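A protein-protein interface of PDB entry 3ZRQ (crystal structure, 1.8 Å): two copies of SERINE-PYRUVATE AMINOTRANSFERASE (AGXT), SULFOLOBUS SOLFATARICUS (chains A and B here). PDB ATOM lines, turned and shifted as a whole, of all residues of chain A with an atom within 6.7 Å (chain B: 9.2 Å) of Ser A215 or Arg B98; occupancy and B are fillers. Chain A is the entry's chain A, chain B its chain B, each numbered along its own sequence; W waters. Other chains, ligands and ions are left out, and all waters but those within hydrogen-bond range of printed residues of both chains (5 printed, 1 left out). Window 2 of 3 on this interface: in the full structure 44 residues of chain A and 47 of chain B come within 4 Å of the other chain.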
ATOM      1  N   THR A  71       2.836 -11.759  -7.489  1.00  0.00           N
ATOM      2  CA  THR A  71       3.746 -10.981  -8.360  1.00  0.00           C
ATOM      3  C   THR A  71       4.818 -10.188  -7.569  1.00  0.00           C
ATOM      4  O   THR A  71       5.867  -9.812  -8.132  1.00  0.00           O
ATOM      5  CB  THR A  71       3.011 -10.019  -9.304  1.00  0.00           C
ATOM      6  OG1 THR A  71       2.247  -9.052  -8.544  1.00  0.00           O
ATOM      7  CG2 THR A  71       2.137 -10.794 -10.294  1.00  0.00           C
ATOM      8  N   SER A  72       4.562  -9.974  -6.279  1.00  0.00           N
ATOM      9  CA  SER A  72       5.540  -9.341  -5.377  1.00  0.00           C
ATOM     10  C   SER A  72       6.846 -10.151  -5.306  1.00  0.00           C
ATOM     11  O   SER A  72       7.882  -9.638  -4.835  1.00  0.00           O
ATOM     12  CB  SER A  72       4.949  -9.176  -3.963  1.00  0.00           C
ATOM     13  OG  SER A  72       3.755  -8.386  -3.992  1.00  0.00           O
ATOM     14  N   LEU A  73       6.797 -11.413  -5.740  1.00  0.00           N
ATOM     15  CA  LEU A  73       7.961 -12.314  -5.624  1.00  0.00           C
ATOM     16  C   LEU A  73       8.675 -12.548  -6.950  1.00  0.00           C
ATOM     17  O   LEU A  73       9.612 -13.373  -7.024  1.00  0.00           O
ATOM     18  CB  LEU A  73       7.532 -13.667  -5.044  1.00  0.00           C
ATOM     19  CG  LEU A  73       6.918 -13.608  -3.643  1.00  0.00           C
ATOM     20  CD1 LEU A  73       6.456 -15.006  -3.212  1.00  0.00           C
ATOM     21  CD2 LEU A  73       7.879 -12.989  -2.624  1.00  0.00           C
ATOM     22  N   LEU A  74       8.211 -11.852  -7.982  1.00  0.00           N
ATOM     23  CA  LEU A  74       8.629 -12.075  -9.369  1.00  0.00           C
ATOM     24  C   LEU A  74       9.397 -10.917 -10.012  1.00  0.00           C
ATOM     25  O   LEU A  74       9.222  -9.743  -9.641  1.00  0.00           O
ATOM     26  CB  LEU A  74       7.412 -12.426 -10.249  1.00  0.00           C
ATOM     27  CG  LEU A  74       6.620 -13.693  -9.801  1.00  0.00           C
ATOM     28  CD1 LEU A  74       5.327 -13.894 -10.581  1.00  0.00           C
ATOM     29  CD2 LEU A  74       7.481 -14.957  -9.834  1.00  0.00           C
ATOM     30  N   LYS A  75      10.212 -11.270 -11.010  1.00  0.00           N
ATOM     31  CA  LYS A  75      10.953 -10.317 -11.856  1.00  0.00           C
ATOM     32  C   LYS A  75      10.656 -10.510 -13.346  1.00  0.00           C
ATOM     33  O   LYS A  75      10.159 -11.583 -13.741  1.00  0.00           O
ATOM     34  CB  LYS A  75      12.451 -10.452 -11.569  1.00  0.00           C
ATOM     35  CG  LYS A  75      12.782  -9.971 -10.177  1.00  0.00           C
ATOM     36  CD  LYS A  75      14.240 -10.051  -9.865  1.00  0.00           C
ATOM     37  CE  LYS A  75      14.565  -9.069  -8.757  1.00  0.00           C
ATOM     38  NZ  LYS A  75      15.813  -9.481  -8.072  1.00  0.00           N
ATOM     39  N   PRO A  76      10.957  -9.491 -14.191  1.00  0.00           N
ATOM     40  CA  PRO A  76      10.589  -9.655 -15.605  1.00  0.00           C
ATOM     41  C   PRO A  76      11.303 -10.906 -16.169  1.00  0.00           C
ATOM     42  O   PRO A  76      12.436 -11.204 -15.758  1.00  0.00           O
ATOM     43  CB  PRO A  76      11.082  -8.361 -16.267  1.00  0.00           C
ATOM     44  CG  PRO A  76      11.179  -7.374 -15.134  1.00  0.00           C
ATOM     45  CD  PRO A  76      11.607  -8.187 -13.943  1.00  0.00           C
ATOM     46  N   ILE A 209      12.926 -12.526  -0.225  1.00  0.00           N
ATOM     47  CA  ILE A 209      12.700 -11.831  -1.487  1.00  0.00           C
ATOM     48  C   ILE A 209      12.065 -10.449  -1.252  1.00  0.00           C
ATOM     49  O   ILE A 209      12.505  -9.447  -1.838  1.00  0.00           O
ATOM     50  CB  ILE A 209      11.824 -12.673  -2.453  1.00  0.00           C
ATOM     51  CG1 ILE A 209      12.578 -13.927  -2.901  1.00  0.00           C
ATOM     52  CG2 ILE A 209      11.360 -11.827  -3.659  1.00  0.00           C
ATOM     53  CD1 ILE A 209      11.804 -14.853  -3.813  1.00  0.00           C
ATOM     54  N   LEU A 210      11.023 -10.388  -0.420  1.00  0.00           N
ATOM     55  CA  LEU A 210      10.349  -9.104  -0.164  1.00  0.00           C
ATOM     56  C   LEU A 210      11.308  -8.090   0.462  1.00  0.00           C
ATOM     57  O   LEU A 210      11.316  -6.928   0.079  1.00  0.00           O
ATOM     58  CB  LEU A 210       9.139  -9.287   0.769  1.00  0.00           C
ATOM     59  CG  LEU A 210       7.954 -10.152   0.296  1.00  0.00           C
ATOM     60  CD1 LEU A 210       6.855 -10.100   1.398  1.00  0.00           C
ATOM     61  CD2 LEU A 210       7.438  -9.647  -1.069  1.00  0.00           C
ATOM     62  N   GLN A 213      14.704  -7.618  -2.520  1.00  0.00           N
ATOM     63  CA  GLN A 213      14.637  -7.507  -3.979  1.00  0.00           C
ATOM     64  C   GLN A 213      13.517  -6.589  -4.455  1.00  0.00           C
ATOM     65  O   GLN A 213      12.534  -6.380  -3.737  1.00  0.00           O
ATOM     66  CB  GLN A 213      14.472  -8.887  -4.623  1.00  0.00           C
ATOM     67  CG  GLN A 213      15.469  -9.950  -4.137  1.00  0.00           C
ATOM     68  CD  GLN A 213      15.453 -11.206  -4.985  1.00  0.00           C
ATOM     69  OE1 GLN A 213      15.206 -11.155  -6.185  1.00  0.00           O
ATOM     70  NE2 GLN A 213      15.715 -12.345  -4.359  1.00  0.00           N
ATOM     71  N   ASN A 214      13.678  -6.053  -5.672  1.00  0.00           N
ATOM     72  CA  ASN A 214      12.605  -5.357  -6.404  1.00  0.00           C
ATOM     73  C   ASN A 214      11.640  -6.395  -6.982  1.00  0.00           C
ATOM     74  O   ASN A 214      11.955  -7.572  -6.986  1.00  0.00           O
ATOM     75  CB  ASN A 214      13.187  -4.558  -7.570  1.00  0.00           C
ATOM     76  CG  ASN A 214      14.076  -3.418  -7.122  1.00  0.00           C
ATOM     77  OD1 ASN A 214      13.916  -2.866  -6.030  1.00  0.00           O
ATOM     78  ND2 ASN A 214      15.019  -3.049  -7.978  1.00  0.00           N
ATOM     79  N   SER A 215      10.494  -5.973  -7.512  1.00  0.00           N
ATOM     80  CA  SER A 215       9.556  -6.939  -8.121  1.00  0.00           C
ATOM     81  C   SER A 215       8.761  -6.232  -9.196  1.00  0.00           C
ATOM     82  O   SER A 215       8.840  -5.013  -9.323  1.00  0.00           O
ATOM     83  CB  SER A 215       8.557  -7.472  -7.080  1.00  0.00           C
ATOM     84  OG  SER A 215       7.569  -6.463  -6.802  1.00  0.00           O
ATOM     85  N   ILE A 216       7.952  -7.003  -9.912  1.00  0.00           N
ATOM     86  CA  ILE A 216       7.052  -6.465 -10.910  1.00  0.00           C
ATOM     87  C   ILE A 216       5.658  -6.072 -10.365  1.00  0.00           C
ATOM     88  O   ILE A 216       4.760  -5.713 -11.151  1.00  0.00           O
ATOM     89  CB  ILE A 216       6.890  -7.462 -12.087  1.00  0.00           C
ATOM     90  CG1 ILE A 216       6.224  -8.769 -11.613  1.00  0.00           C
ATOM     91  CG2 ILE A 216       8.276  -7.703 -12.780  1.00  0.00           C
ATOM     92  CD1 ILE A 216       6.150  -9.831 -12.691  1.00  0.00           C
ATOM     93  N   ALA A 217       5.480  -6.124  -9.048  1.00  0.00           N
ATOM     94  CA  ALA A 217       4.166  -5.814  -8.445  1.00  0.00           C
ATOM     95  C   ALA A 217       3.722  -4.387  -8.721  1.00  0.00           C
ATOM     96  O   ALA A 217       4.552  -3.507  -8.988  1.00  0.00           O
ATOM     97  CB  ALA A 217       4.189  -6.066  -6.955  1.00  0.00           C
ATOM     98  N   GLY A 218       2.411  -4.165  -8.681  1.00  0.00           N
ATOM     99  CA  GLY A 218       1.837  -2.811  -8.732  1.00  0.00           C
ATOM    100  C   GLY A 218       1.998  -2.152  -7.373  1.00  0.00           C
ATOM    101  O   GLY A 218       2.961  -2.418  -6.666  1.00  0.00           O
ATOM    102  N   TYR A 219       1.059  -1.295  -6.984  1.00  0.00           N
ATOM    103  CA  TYR A 219       1.205  -0.570  -5.718  1.00  0.00           C
ATOM    104  C   TYR A 219       0.397  -1.231  -4.581  1.00  0.00           C
ATOM    105  O   TYR A 219       0.954  -1.725  -3.586  1.00  0.00           O
ATOM    106  CB  TYR A 219       0.826   0.914  -5.917  1.00  0.00           C
ATOM    107  CG  TYR A 219       1.132   1.809  -4.729  1.00  0.00           C
ATOM    108  CD1 TYR A 219       2.458   2.162  -4.415  1.00  0.00           C
ATOM    109  CD2 TYR A 219       0.106   2.264  -3.898  1.00  0.00           C
ATOM    110  CE1 TYR A 219       2.739   2.989  -3.319  1.00  0.00           C
ATOM    111  CE2 TYR A 219       0.381   3.089  -2.798  1.00  0.00           C
ATOM    112  CZ  TYR A 219       1.692   3.435  -2.520  1.00  0.00           C
ATOM    113  OH  TYR A 219       1.940   4.246  -1.441  1.00  0.00           O
ATOM    114  N   TYR A 220      -0.919  -1.273  -4.756  1.00  0.00           N
ATOM    115  CA  TYR A 220      -1.843  -1.820  -3.754  1.00  0.00           C
ATOM    116  C   TYR A 220      -1.545  -3.283  -3.406  1.00  0.00           C
ATOM    117  O   TYR A 220      -1.700  -3.701  -2.251  1.00  0.00           O
ATOM    118  CB  TYR A 220      -3.277  -1.680  -4.261  1.00  0.00           C
ATOM    119  CG  TYR A 220      -4.339  -1.709  -3.159  1.00  0.00           C
ATOM    120  CD1 TYR A 220      -4.469  -0.636  -2.265  1.00  0.00           C
ATOM    121  CD2 TYR A 220      -5.256  -2.751  -3.074  1.00  0.00           C
ATOM    122  CE1 TYR A 220      -5.451  -0.625  -1.256  1.00  0.00           C
ATOM    123  CE2 TYR A 220      -6.261  -2.753  -2.083  1.00  0.00           C
ATOM    124  CZ  TYR A 220      -6.354  -1.700  -1.178  1.00  0.00           C
ATOM    125  OH  TYR A 220      -7.337  -1.690  -0.188  1.00  0.00           O
ATOM    126  N   ASP A 222       1.454  -4.946  -3.848  1.00  0.00           N
ATOM    127  CA  ASP A 222       2.832  -5.240  -3.451  1.00  0.00           C
ATOM    128  C   ASP A 222       2.849  -5.574  -1.952  1.00  0.00           C
ATOM    129  O   ASP A 222       2.558  -4.715  -1.086  1.00  0.00           O
ATOM    130  CB  ASP A 222       3.738  -4.044  -3.768  1.00  0.00           C
ATOM    131  CG  ASP A 222       5.251  -4.336  -3.522  1.00  0.00           C
ATOM    132  OD1 ASP A 222       5.614  -5.376  -2.904  1.00  0.00           O
ATOM    133  OD2 ASP A 222       6.064  -3.494  -3.980  1.00  0.00           O
ATOM    134  N   ARG A 224       5.192  -5.908   0.027  1.00  0.00           N
ATOM    135  CA  ARG A 224       6.169  -5.064   0.780  1.00  0.00           C
ATOM    136  C   ARG A 224       5.471  -3.884   1.461  1.00  0.00           C
ATOM    137  O   ARG A 224       5.869  -3.460   2.544  1.00  0.00           O
ATOM    138  CB  ARG A 224       7.292  -4.549  -0.134  1.00  0.00           C
ATOM    139  CG  ARG A 224       8.228  -5.628  -0.645  1.00  0.00           C
ATOM    140  CD  ARG A 224       9.064  -5.108  -1.803  1.00  0.00           C
ATOM    141  NE  ARG A 224       9.849  -6.194  -2.382  1.00  0.00           N
ATOM    142  CZ  ARG A 224       9.354  -7.077  -3.244  1.00  0.00           C
ATOM    143  NH1 ARG A 224       8.077  -6.984  -3.645  1.00  0.00           N
ATOM    144  NH2 ARG A 224      10.133  -8.030  -3.725  1.00  0.00           N
ATOM    145  N   ASN A 225       4.415  -3.371   0.825  1.00  0.00           N
ATOM    146  CA  ASN A 225       3.641  -2.261   1.386  1.00  0.00           C
ATOM    147  C   ASN A 225       2.772  -2.625   2.593  1.00  0.00           C
ATOM    148  O   ASN A 225       2.484  -1.759   3.437  1.00  0.00           O
ATOM    149  CB  ASN A 225       2.790  -1.597   0.311  1.00  0.00           C
ATOM    150  CG  ASN A 225       3.602  -0.760  -0.660  1.00  0.00           C
ATOM    151  OD1 ASN A 225       4.600  -0.168  -0.273  1.00  0.00           O
ATOM    152  ND2 ASN A 225       3.133  -0.647  -1.921  1.00  0.00           N
ATOM    153  N   GLU B  68      -5.465   3.444  -7.996  1.00  0.00           N
ATOM    154  CA  GLU B  68      -4.663   2.568  -8.866  1.00  0.00           C
ATOM    155  C   GLU B  68      -5.470   2.076 -10.114  1.00  0.00           C
ATOM    156  O   GLU B  68      -4.932   1.982 -11.212  1.00  0.00           O
ATOM    157  CB  GLU B  68      -4.008   1.434  -8.060  1.00  0.00           C
ATOM    158  CG  GLU B  68      -3.015   0.572  -8.862  1.00  0.00           C
ATOM    159  CD  GLU B  68      -2.078  -0.200  -7.982  1.00  0.00           C
ATOM    160  OE1 GLU B  68      -2.139  -0.055  -6.737  1.00  0.00           O
ATOM    161  OE2 GLU B  68      -1.261  -0.967  -8.529  1.00  0.00           O
ATOM    162  N   THR B  71      -5.266   3.366 -13.766  1.00  0.00           N
ATOM    163  CA  THR B  71      -4.358   2.777 -14.772  1.00  0.00           C
ATOM    164  C   THR B  71      -5.111   2.019 -15.887  1.00  0.00           C
ATOM    165  O   THR B  71      -4.562   1.796 -16.987  1.00  0.00           O
ATOM    166  CB  THR B  71      -3.281   1.847 -14.170  1.00  0.00           C
ATOM    167  OG1 THR B  71      -3.902   0.755 -13.464  1.00  0.00           O
ATOM    168  CG2 THR B  71      -2.343   2.604 -13.213  1.00  0.00           C
ATOM    169  N   ARG B  91       0.516  10.389  -3.235  1.00  0.00           N
ATOM    170  CA  ARG B  91       0.203   8.967  -3.463  1.00  0.00           C
ATOM    171  C   ARG B  91      -0.027   8.655  -4.939  1.00  0.00           C
ATOM    172  O   ARG B  91       0.327   7.566  -5.391  1.00  0.00           O
ATOM    173  CB  ARG B  91      -0.985   8.513  -2.598  1.00  0.00           C
ATOM    174  CG  ARG B  91      -1.376   7.024  -2.797  1.00  0.00           C
ATOM    175  CD  ARG B  91      -2.116   6.529  -1.592  1.00  0.00           C
ATOM    176  NE  ARG B  91      -1.157   6.332  -0.513  1.00  0.00           N
ATOM    177  CZ  ARG B  91      -1.351   5.587   0.566  1.00  0.00           C
ATOM    178  NH1 ARG B  91      -2.497   4.920   0.765  1.00  0.00           N
ATOM    179  NH2 ARG B  91      -0.382   5.503   1.455  1.00  0.00           N
ATOM    180  N   TRP B  92      -0.631   9.570  -5.695  1.00  0.00           N
ATOM    181  CA  TRP B  92      -0.757   9.378  -7.139  1.00  0.00           C
ATOM    182  C   TRP B  92       0.604   9.086  -7.790  1.00  0.00           C
ATOM    183  O   TRP B  92       0.739   8.153  -8.592  1.00  0.00           O
ATOM    184  CB  TRP B  92      -1.364  10.584  -7.832  1.00  0.00           C
ATOM    185  CG  TRP B  92      -2.844  10.813  -7.715  1.00  0.00           C
ATOM    186  CD1 TRP B  92      -3.452  11.884  -7.119  1.00  0.00           C
ATOM    187  CD2 TRP B  92      -3.893  10.010  -8.267  1.00  0.00           C
ATOM    188  NE1 TRP B  92      -4.811  11.806  -7.268  1.00  0.00           N
ATOM    189  CE2 TRP B  92      -5.112  10.654  -7.960  1.00  0.00           C
ATOM    190  CE3 TRP B  92      -3.923   8.785  -8.956  1.00  0.00           C
ATOM    191  CZ2 TRP B  92      -6.354  10.122  -8.321  1.00  0.00           C
ATOM    192  CZ3 TRP B  92      -5.181   8.258  -9.355  1.00  0.00           C
ATOM    193  CH2 TRP B  92      -6.368   8.930  -9.037  1.00  0.00           C
ATOM    194  N   GLU B  93       1.611   9.872  -7.427  1.00  0.00           N
ATOM    195  CA  GLU B  93       2.974   9.654  -7.948  1.00  0.00           C
ATOM    196  C   GLU B  93       3.562   8.317  -7.513  1.00  0.00           C
ATOM    197  O   GLU B  93       4.179   7.634  -8.319  1.00  0.00           O
ATOM    198  CB  GLU B  93       3.905  10.802  -7.517  1.00  0.00           C
ATOM    199  CG  GLU B  93       5.366  10.634  -7.950  1.00  0.00           C
ATOM    200  CD  GLU B  93       6.234  11.842  -7.542  1.00  0.00           C
ATOM    201  OE1 GLU B  93       6.138  12.325  -6.388  1.00  0.00           O
ATOM    202  OE2 GLU B  93       7.029  12.302  -8.383  1.00  0.00           O
ATOM    203  N   GLN B  94       3.375   7.963  -6.243  1.00  0.00           N
ATOM    204  CA  GLN B  94       3.816   6.682  -5.702  1.00  0.00           C
ATOM    205  C   GLN B  94       3.192   5.461  -6.435  1.00  0.00           C
ATOM    206  O   GLN B  94       3.902   4.491  -6.745  1.00  0.00           O
ATOM    207  CB  GLN B  94       3.567   6.615  -4.192  1.00  0.00           C
ATOM    208  CG  GLN B  94       4.403   7.584  -3.356  1.00  0.00           C
ATOM    209  CD  GLN B  94       5.904   7.339  -3.498  1.00  0.00           C
ATOM    210  OE1 GLN B  94       6.646   8.187  -4.005  1.00  0.00           O
ATOM    211  NE2 GLN B  94       6.348   6.166  -3.083  1.00  0.00           N
ATOM    212  N   ILE B  95       1.896   5.538  -6.742  1.00  0.00           N
ATOM    213  CA  ILE B  95       1.202   4.502  -7.544  1.00  0.00           C
ATOM    214  C   ILE B  95       1.757   4.462  -8.983  1.00  0.00           C
ATOM    215  O   ILE B  95       2.145   3.397  -9.488  1.00  0.00           O
ATOM    216  CB  ILE B  95      -0.318   4.822  -7.642  1.00  0.00           C
ATOM    217  CG1 ILE B  95      -0.992   4.726  -6.273  1.00  0.00           C
ATOM    218  CG2 ILE B  95      -1.034   3.901  -8.715  1.00  0.00           C
ATOM    219  CD1 ILE B  95      -2.376   5.295  -6.253  1.00  0.00           C
ATOM    220  N   PHE B  96       1.762   5.624  -9.649  1.00  0.00           N
ATOM    221  CA  PHE B  96       2.227   5.714 -11.038  1.00  0.00           C
ATOM    222  C   PHE B  96       3.709   5.373 -11.235  1.00  0.00           C
ATOM    223  O   PHE B  96       4.100   4.968 -12.329  1.00  0.00           O
ATOM    224  CB  PHE B  96       1.872   7.070 -11.642  1.00  0.00           C
ATOM    225  CG  PHE B  96       0.398   7.282 -11.810  1.00  0.00           C
ATOM    226  CD1 PHE B  96      -0.425   6.238 -12.257  1.00  0.00           C
ATOM    227  CD2 PHE B  96      -0.176   8.523 -11.536  1.00  0.00           C
ATOM    228  CE1 PHE B  96      -1.792   6.440 -12.443  1.00  0.00           C
ATOM    229  CE2 PHE B  96      -1.533   8.729 -11.697  1.00  0.00           C
ATOM    230  CZ  PHE B  96      -2.347   7.688 -12.162  1.00  0.00           C
ATOM    231  N   LYS B  97       4.514   5.455 -10.171  1.00  0.00           N
ATOM    232  CA  LYS B  97       5.915   4.967 -10.232  1.00  0.00           C
ATOM    233  C   LYS B  97       6.024   3.471 -10.559  1.00  0.00           C
ATOM    234  O   LYS B  97       7.062   3.003 -11.056  1.00  0.00           O
ATOM    235  CB  LYS B  97       6.685   5.278  -8.949  1.00  0.00           C
ATOM    236  CG  LYS B  97       7.274   6.705  -8.987  1.00  0.00           C
ATOM    237  CD  LYS B  97       8.207   7.045  -7.855  1.00  0.00           C
ATOM    238  CE  LYS B  97       8.885   8.393  -8.175  1.00  0.00           C
ATOM    239  NZ  LYS B  97       9.270   9.184  -6.957  1.00  0.00           N
ATOM    240  N   ARG B  98       4.959   2.727 -10.276  1.00  0.00           N
ATOM    241  CA  ARG B  98       4.944   1.276 -10.557  1.00  0.00           C
ATOM    242  C   ARG B  98       4.556   0.933 -12.001  1.00  0.00           C
ATOM    243  O   ARG B  98       4.562  -0.244 -12.381  1.00  0.00           O
ATOM    244  CB  ARG B  98       4.007   0.551  -9.563  1.00  0.00           C
ATOM    245  CG  ARG B  98       4.308   0.782  -8.059  1.00  0.00           C
ATOM    246  CD  ARG B  98       5.714   0.421  -7.647  1.00  0.00           C
ATOM    247  NE  ARG B  98       5.986  -1.001  -7.867  1.00  0.00           N
ATOM    248  CZ  ARG B  98       7.178  -1.586  -7.736  1.00  0.00           C
ATOM    249  NH1 ARG B  98       8.259  -0.888  -7.403  1.00  0.00           N
ATOM    250  NH2 ARG B  98       7.298  -2.889  -7.944  1.00  0.00           N
ATOM    251  N   TYR B  99       4.209   1.942 -12.801  1.00  0.00           N
ATOM    252  CA  TYR B  99       3.643   1.749 -14.141  1.00  0.00           C
ATOM    253  C   TYR B  99       4.501   2.458 -15.190  1.00  0.00           C
ATOM    254  O   TYR B  99       5.211   3.404 -14.837  1.00  0.00           O
ATOM    255  CB  TYR B  99       2.194   2.254 -14.173  1.00  0.00           C
ATOM    256  CG  TYR B  99       1.275   1.360 -13.344  1.00  0.00           C
ATOM    257  CD1 TYR B  99       1.139   1.543 -11.970  1.00  0.00           C
ATOM    258  CD2 TYR B  99       0.607   0.277 -13.942  1.00  0.00           C
ATOM    259  CE1 TYR B  99       0.310   0.692 -11.193  1.00  0.00           C
ATOM    260  CE2 TYR B  99      -0.214  -0.561 -13.198  1.00  0.00           C
ATOM    261  CZ  TYR B  99      -0.357  -0.359 -11.831  1.00  0.00           C
ATOM    262  OH  TYR B  99      -1.148  -1.222 -11.116  1.00  0.00           O
ATOM    263  N   PRO B 100       4.448   2.003 -16.465  1.00  0.00           N
ATOM    264  CA  PRO B 100       5.311   2.583 -17.520  1.00  0.00           C
ATOM    265  C   PRO B 100       4.739   3.892 -18.023  1.00  0.00           C
ATOM    266  O   PRO B 100       4.296   3.978 -19.171  1.00  0.00           O
ATOM    267  CB  PRO B 100       5.268   1.529 -18.632  1.00  0.00           C
ATOM    268  CG  PRO B 100       3.940   0.823 -18.420  1.00  0.00           C
ATOM    269  CD  PRO B 100       3.769   0.778 -16.927  1.00  0.00           C
ATOM    270  N   VAL B 101       4.720   4.906 -17.155  1.00  0.00           N
ATOM    271  CA  VAL B 101       4.115   6.179 -17.520  1.00  0.00           C
ATOM    272  C   VAL B 101       5.023   7.327 -17.106  1.00  0.00           C
ATOM    273  O   VAL B 101       5.906   7.139 -16.280  1.00  0.00           O
ATOM    274  CB  VAL B 101       2.721   6.361 -16.863  1.00  0.00           C
ATOM    275  CG1 VAL B 101       1.693   5.358 -17.464  1.00  0.00           C
ATOM    276  CG2 VAL B 101       2.834   6.230 -15.353  1.00  0.00           C
ATOM    277  N   VAL B 103       5.351  10.953 -15.321  1.00  0.00           N
ATOM    278  CA  VAL B 103       4.660  11.773 -14.321  1.00  0.00           C
ATOM    279  C   VAL B 103       5.375  13.094 -13.976  1.00  0.00           C
ATOM    280  O   VAL B 103       6.544  13.101 -13.578  1.00  0.00           O
ATOM    281  CB  VAL B 103       4.479  10.979 -13.016  1.00  0.00           C
ATOM    282  CG1 VAL B 103       3.655  11.793 -11.993  1.00  0.00           C
ATOM    283  CG2 VAL B 103       3.837   9.623 -13.306  1.00  0.00           C
ATOM    284  N   ILE B 216      -2.617  -0.580 -19.376  1.00  0.00           N
ATOM    285  CA  ILE B 216      -1.525  -1.080 -18.559  1.00  0.00           C
ATOM    286  C   ILE B 216      -1.960  -1.668 -17.205  1.00  0.00           C
ATOM    287  O   ILE B 216      -1.105  -2.013 -16.364  1.00  0.00           O
ATOM    288  CB  ILE B 216      -0.432  -0.005 -18.355  1.00  0.00           C
ATOM    289  CG1 ILE B 216      -0.994   1.174 -17.533  1.00  0.00           C
ATOM    290  CG2 ILE B 216       0.122   0.438 -19.739  1.00  0.00           C
ATOM    291  CD1 ILE B 216      -0.050   2.338 -17.357  1.00  0.00           C
ATOM    292  N   ALA B 217      -3.265  -1.795 -16.991  1.00  0.00           N
ATOM    293  CA  ALA B 217      -3.766  -2.284 -15.688  1.00  0.00           C
ATOM    294  C   ALA B 217      -3.307  -3.726 -15.407  1.00  0.00           C
ATOM    295  O   ALA B 217      -2.970  -4.467 -16.321  1.00  0.00           O
ATOM    296  CB  ALA B 217      -5.263  -2.190 -15.622  1.00  0.00           C
ATOM    297  N   GLY B 218      -3.265  -4.080 -14.135  1.00  0.00           N
ATOM    298  CA  GLY B 218      -3.081  -5.467 -13.696  1.00  0.00           C
ATOM    299  C   GLY B 218      -4.386  -6.226 -13.908  1.00  0.00           C
ATOM    300  O   GLY B 218      -5.159  -5.940 -14.829  1.00  0.00           O
HETATM  301  O   HOH W   1      -1.336  -3.481  -7.424  1.00  0.00           O
HETATM  302  O   HOH W   2       5.009   4.711  -1.223  1.00  0.00           O
HETATM  303  O   HOH W   3       8.304  -4.359  -5.372  1.00  0.00           O
HETATM  304  O   HOH W   4       5.092  -1.288  -4.840  1.00  0.00           O
HETATM  305  O   HOH W   5      10.404  -2.790  -7.207  1.00  0.00           O
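Printed residues of chain B that touch a printed residue of chain A: Glu B68, Arg B91, Gln B94, Ile B95 and Arg B98.
Printed residues of chain A that touch a printed residue of chain B: Ser A215, Ala A217, Gly A218, Tyr A219 and Tyr A220.
Hydrophobic or aromatic side chains of chain A that line the printed part of chain B: Tyr A219 and Tyr A220.
Ser A72 touches none of the printed residues of chain B.
Ala A217 touches just one residue of chain B: Arg B98.
Gly A218 touches just these residues of chain B: Glu B68 (3.6 Å) and Arg B98 (3.5 Å).
Of the printed residues of chain A, Ile B95 touches Tyr A219.
Printed residues of chain B within 4 Å of Tyr A220: Glu B68.
Asn A225 touches none of the printed residues of chain B.
Asn A214 touches none of the printed residues of chain B.
The nearest printed residue of chain A that does not touch Ile B95 is Gly A218 (5.9 Å).
Glu B68 touches Gly A218.
Arg B98 touches Gly A218 (NE to O, 3.5 Å).
NE of Arg B91 touches OH of Tyr A219, 3.8 Å away.
O of Gln B94 touches CD1 of Tyr A219, 3.6 Å away.
Tyr A219 touches Ile B95 (CD2 to CG1, 3.6 Å).
4 positions are printed for both chains.
The side-chain hydroxyl of Ser A215 sits at hydrogen-bond distance from the backbone NH of Ala A217 (3.1 Å).
NH1 of Arg A224 sits at hydrogen-bond distance from OG of Ser A215, 3.2 Å away.
The side-chain amide nitrogen (ND2) of Asn A225 sits at hydrogen-bond distance from the backbone carbonyl oxygen (O) of Tyr A219 (2.9 Å).
The backbone carbonyl oxygen (O) of Glu B68 lies within hydrogen-bond range of the side-chain hydroxyl (OG1) of Thr B71, 2.8 Å away.
OE2 of Glu B68 sits at hydrogen-bond distance from OH of Tyr B99 (2.6 Å).
Water W4 lies within hydrogen-bond range of OD2 of Asp A222 (2.6 Å), O of Gly A218 (3.0 Å) and NE of Arg B98 (3.2 Å).
Water W3 lies within hydrogen-bond range of the side-chain hydroxyl (OG) of Ser A215, the side-chain carboxylate (OD2) of Asp A222, the guanidinium group (NH2) of Arg B98 and the guanidinium group (NH1) of Arg A224.
Water W2 lies within hydrogen-bond range of NE2 of Gln B94 (2.7 Å) and OH of Tyr A219 (3.1 Å).
Water W1 lies within hydrogen-bond range of the side-chain carboxylate of Glu B68 (2.7 Å), the backbone NH of Tyr A219 (3.3 Å) and the backbone NH of Tyr A220 (3.5 Å).
Water W5 lies within hydrogen-bond range of NH1 of Arg B98 (2.9 Å) and N of Ser A215 (3.2 Å).
The guanidinium group (NH2) of Arg B98 is in hydrogen-bond range of the backbone carbonyl oxygen (O) of Ser A215.
NH2 of Arg B98 sits at hydrogen-bond distance from O of Ala A217 (3.0 Å).
The backbone NH of Tyr A219 lies within hydrogen-bond range of the side-chain carboxylate of Glu B68.
N of Tyr A220 is in hydrogen-bond range of OE1 of Glu B68 (2.6 Å).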
